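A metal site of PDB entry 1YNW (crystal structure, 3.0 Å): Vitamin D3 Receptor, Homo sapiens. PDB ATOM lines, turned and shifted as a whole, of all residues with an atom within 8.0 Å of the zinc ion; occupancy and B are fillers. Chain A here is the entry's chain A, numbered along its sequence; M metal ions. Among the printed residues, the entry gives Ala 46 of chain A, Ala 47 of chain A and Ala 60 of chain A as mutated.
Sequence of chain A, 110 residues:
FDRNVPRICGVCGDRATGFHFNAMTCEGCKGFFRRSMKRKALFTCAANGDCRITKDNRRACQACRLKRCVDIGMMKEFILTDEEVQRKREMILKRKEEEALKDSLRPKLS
The side-chain sulfur (SG) of Cys 64 lies close to the backbone NH (N) of Asp 50 (3.4 Å). SG of Cys 45 sits close to N of Gly 49. SG of Cys 45 sits close to N of Ala 47 (3.5 Å).
Merely in contact with the zinc ion: Asp 50. Within 4 Å of the zinc ion: Cys 45, Asp 50, Cys 51, Cys 61 and Cys 64. The nearest printed residue that does not touch the zinc ion is Gly 49 (4.1 Å).
The zinc ion is bound by SG of Cys 51 (2.3 Å), SG of Cys 61 (2.4 Å), SG of Cys 64 (2.4 Å) and SG of Cys 45 (2.4 Å).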
ATOM      1  N   THR A  44       0.745  12.550  20.291  1.00  0.00           N
ATOM      2  CA  THR A  44      -0.485  12.025  19.683  1.00  0.00           C
ATOM      3  C   THR A  44      -0.506  12.498  18.225  1.00  0.00           C
ATOM      4  O   THR A  44      -0.465  13.693  17.918  1.00  0.00           O
ATOM      5  CB  THR A  44      -1.747  12.503  20.422  1.00  0.00           C
ATOM      6  OG1 THR A  44      -1.815  13.932  20.356  1.00  0.00           O
ATOM      7  CG2 THR A  44      -1.694  12.101  21.893  1.00  0.00           C
ATOM      8  N   CYS A  45      -0.540  11.532  17.328  1.00  0.00           N
ATOM      9  CA  CYS A  45      -0.506  11.782  15.901  1.00  0.00           C
ATOM     10  C   CYS A  45      -1.807  12.337  15.342  1.00  0.00           C
ATOM     11  O   CYS A  45      -2.850  11.697  15.467  1.00  0.00           O
ATOM     12  CB  CYS A  45      -0.127  10.460  15.223  1.00  0.00           C
ATOM     13  SG  CYS A  45      -0.975  10.057  13.723  1.00  0.00           S
ATOM     14  N   ALA A  46      -1.768  13.523  14.719  1.00  0.00           N
ATOM     15  CA  ALA A  46      -3.001  14.095  14.140  1.00  0.00           C
ATOM     16  C   ALA A  46      -3.621  13.078  13.184  1.00  0.00           C
ATOM     17  O   ALA A  46      -4.785  12.733  13.316  1.00  0.00           O
ATOM     18  CB  ALA A  46      -2.719  15.413  13.400  1.00  0.00           C
ATOM     19  N   ALA A  47      -2.836  12.598  12.224  1.00  0.00           N
ATOM     20  CA  ALA A  47      -3.325  11.633  11.253  1.00  0.00           C
ATOM     21  C   ALA A  47      -3.988  10.414  11.896  1.00  0.00           C
ATOM     22  O   ALA A  47      -4.467  10.477  13.030  1.00  0.00           O
ATOM     23  CB  ALA A  47      -2.183  11.181  10.330  1.00  0.00           C
ATOM     24  N   ASN A  48      -4.009   9.316  11.167  1.00  0.00           N
ATOM     25  CA  ASN A  48      -4.619   8.097  11.683  1.00  0.00           C
ATOM     26  C   ASN A  48      -3.549   7.168  12.205  1.00  0.00           C
ATOM     27  O   ASN A  48      -3.540   5.954  11.910  1.00  0.00           O
ATOM     28  CB  ASN A  48      -5.467   7.394  10.611  1.00  0.00           C
ATOM     29  CG  ASN A  48      -6.927   7.863  10.625  1.00  0.00           C
ATOM     30  OD1 ASN A  48      -7.694   7.484  11.519  1.00  0.00           O
ATOM     31  ND2 ASN A  48      -7.307   8.703   9.659  1.00  0.00           N
ATOM     32  N   GLY A  49      -2.651   7.780  12.988  1.00  0.00           N
ATOM     33  CA  GLY A  49      -1.545   7.082  13.622  1.00  0.00           C
ATOM     34  C   GLY A  49      -0.762   6.159  12.721  1.00  0.00           C
ATOM     35  O   GLY A  49      -0.633   4.965  13.025  1.00  0.00           O
ATOM     36  N   ASP A  50      -0.226   6.691  11.627  1.00  0.00           N
ATOM     37  CA  ASP A  50       0.541   5.824  10.763  1.00  0.00           C
ATOM     38  C   ASP A  50       1.331   6.466   9.648  1.00  0.00           C
ATOM     39  O   ASP A  50       1.453   5.911   8.549  1.00  0.00           O
ATOM     40  CB  ASP A  50      -0.364   4.739  10.187  1.00  0.00           C
ATOM     41  CG  ASP A  50       0.433   3.510   9.778  1.00  0.00           C
ATOM     42  OD1 ASP A  50       1.307   3.077  10.583  1.00  0.00           O
ATOM     43  OD2 ASP A  50       0.180   2.993   8.666  1.00  0.00           O
ATOM     44  N   CYS A  51       1.881   7.636   9.935  1.00  0.00           N
ATOM     45  CA  CYS A  51       2.685   8.326   8.932  1.00  0.00           C
ATOM     46  C   CYS A  51       3.962   7.504   8.665  1.00  0.00           C
ATOM     47  O   CYS A  51       4.279   6.567   9.417  1.00  0.00           O
ATOM     48  CB  CYS A  51       3.087   9.732   9.429  1.00  0.00           C
ATOM     49  SG  CYS A  51       2.268  10.274  10.974  1.00  0.00           S
ATOM     50  N   ARG A  52       4.658   7.832   7.585  1.00  0.00           N
ATOM     51  CA  ARG A  52       5.918   7.159   7.252  1.00  0.00           C
ATOM     52  C   ARG A  52       7.083   8.100   7.596  1.00  0.00           C
ATOM     53  O   ARG A  52       7.174   9.242   7.098  1.00  0.00           O
ATOM     54  CB  ARG A  52       5.978   6.751   5.776  1.00  0.00           C
ATOM     55  CG  ARG A  52       5.054   5.608   5.475  1.00  0.00           C
ATOM     56  CD  ARG A  52       5.258   5.014   4.097  1.00  0.00           C
ATOM     57  NE  ARG A  52       4.131   4.147   3.758  1.00  0.00           N
ATOM     58  CZ  ARG A  52       3.957   3.542   2.577  1.00  0.00           C
ATOM     59  NH1 ARG A  52       4.855   3.698   1.604  1.00  0.00           N
ATOM     60  NH2 ARG A  52       2.884   2.783   2.368  1.00  0.00           N
ATOM     61  N   ILE A  53       7.948   7.606   8.474  1.00  0.00           N
ATOM     62  CA  ILE A  53       9.108   8.370   8.925  1.00  0.00           C
ATOM     63  C   ILE A  53      10.177   8.371   7.830  1.00  0.00           C
ATOM     64  O   ILE A  53      10.517   7.325   7.262  1.00  0.00           O
ATOM     65  CB  ILE A  53       9.695   7.743  10.218  1.00  0.00           C
ATOM     66  CG1 ILE A  53       8.564   7.380  11.196  1.00  0.00           C
ATOM     67  CG2 ILE A  53      10.685   8.734  10.859  1.00  0.00           C
ATOM     68  CD1 ILE A  53       7.836   8.562  11.836  1.00  0.00           C
ATOM     69  N   ALA A  60       7.869  15.858  11.629  1.00  0.00           N
ATOM     70  CA  ALA A  60       6.452  16.155  11.359  1.00  0.00           C
ATOM     71  C   ALA A  60       5.559  15.621  12.449  1.00  0.00           C
ATOM     72  O   ALA A  60       4.978  16.406  13.189  1.00  0.00           O
ATOM     73  CB  ALA A  60       6.044  15.552  10.052  1.00  0.00           C
ATOM     74  N   CYS A  61       5.449  14.289  12.531  1.00  0.00           N
ATOM     75  CA  CYS A  61       4.595  13.607  13.534  1.00  0.00           C
ATOM     76  C   CYS A  61       5.408  12.878  14.639  1.00  0.00           C
ATOM     77  O   CYS A  61       5.810  11.712  14.479  1.00  0.00           O
ATOM     78  CB  CYS A  61       3.675  12.612  12.806  1.00  0.00           C
ATOM     79  SG  CYS A  61       2.369  11.870  13.806  1.00  0.00           S
ATOM     80  N   GLN A  62       5.643  13.544  15.764  1.00  0.00           N
ATOM     81  CA  GLN A  62       6.402  12.943  16.862  1.00  0.00           C
ATOM     82  C   GLN A  62       5.787  11.639  17.332  1.00  0.00           C
ATOM     83  O   GLN A  62       6.439  10.598  17.348  1.00  0.00           O
ATOM     84  CB  GLN A  62       6.492  13.906  18.040  1.00  0.00           C
ATOM     85  CG  GLN A  62       7.151  15.240  17.677  1.00  0.00           C
ATOM     86  CD  GLN A  62       7.160  16.209  18.843  1.00  0.00           C
ATOM     87  OE1 GLN A  62       6.144  16.487  19.459  1.00  0.00           O
ATOM     88  NE2 GLN A  62       8.325  16.730  19.148  1.00  0.00           N
ATOM     89  N   ALA A  63       4.532  11.678  17.722  1.00  0.00           N
ATOM     90  CA  ALA A  63       3.915  10.448  18.165  1.00  0.00           C
ATOM     91  C   ALA A  63       4.353   9.245  17.309  1.00  0.00           C
ATOM     92  O   ALA A  63       4.764   8.200  17.845  1.00  0.00           O
ATOM     93  CB  ALA A  63       2.405  10.595  18.144  1.00  0.00           C
ATOM     94  N   CYS A  64       4.289   9.352  15.997  1.00  0.00           N
ATOM     95  CA  CYS A  64       4.663   8.199  15.190  1.00  0.00           C
ATOM     96  C   CYS A  64       6.170   7.882  15.269  1.00  0.00           C
ATOM     97  O   CYS A  64       6.536   6.699  15.377  1.00  0.00           O
ATOM     98  CB  CYS A  64       4.227   8.394  13.720  1.00  0.00           C
ATOM     99  SG  CYS A  64       2.481   7.844  13.272  1.00  0.00           S
ATOM    100  N   ARG A  65       7.020   8.913  15.228  1.00  0.00           N
ATOM    101  CA  ARG A  65       8.482   8.733  15.321  1.00  0.00           C
ATOM    102  C   ARG A  65       8.752   7.892  16.549  1.00  0.00           C
ATOM    103  O   ARG A  65       9.308   6.777  16.459  1.00  0.00           O
ATOM    104  CB  ARG A  65       9.213  10.082  15.490  1.00  0.00           C
ATOM    105  CG  ARG A  65      10.763  10.004  15.386  1.00  0.00           C
ATOM    106  CD  ARG A  65      11.434  11.407  15.425  1.00  0.00           C
ATOM    107  NE  ARG A  65      12.853  11.368  15.039  1.00  0.00           N
ATOM    108  CZ  ARG A  65      13.659  12.434  15.021  1.00  0.00           C
ATOM    109  NH1 ARG A  65      13.193  13.641  15.371  1.00  0.00           N
ATOM    110  NH2 ARG A  65      14.932  12.318  14.684  1.00  0.00           N
ATOM    111  N   LYS A  67       6.755   6.060  18.505  1.00  0.00           N
ATOM    112  CA  LYS A  67       6.222   4.706  18.394  1.00  0.00           C
ATOM    113  C   LYS A  67       7.099   3.850  17.492  1.00  0.00           C
ATOM    114  O   LYS A  67       7.265   2.639  17.717  1.00  0.00           O
ATOM    115  CB  LYS A  67       4.800   4.698  17.828  1.00  0.00           C
ATOM    116  CG  LYS A  67       4.229   3.290  17.650  1.00  0.00           C
ATOM    117  CD  LYS A  67       3.199   3.292  16.506  1.00  0.00           C
ATOM    118  CE  LYS A  67       2.807   1.882  16.043  1.00  0.00           C
ATOM    119  NZ  LYS A  67       2.219   1.872  14.671  1.00  0.00           N
HETATM  120 ZN    ZN M   1       1.341   9.905  13.020  1.00  0.00          ZN
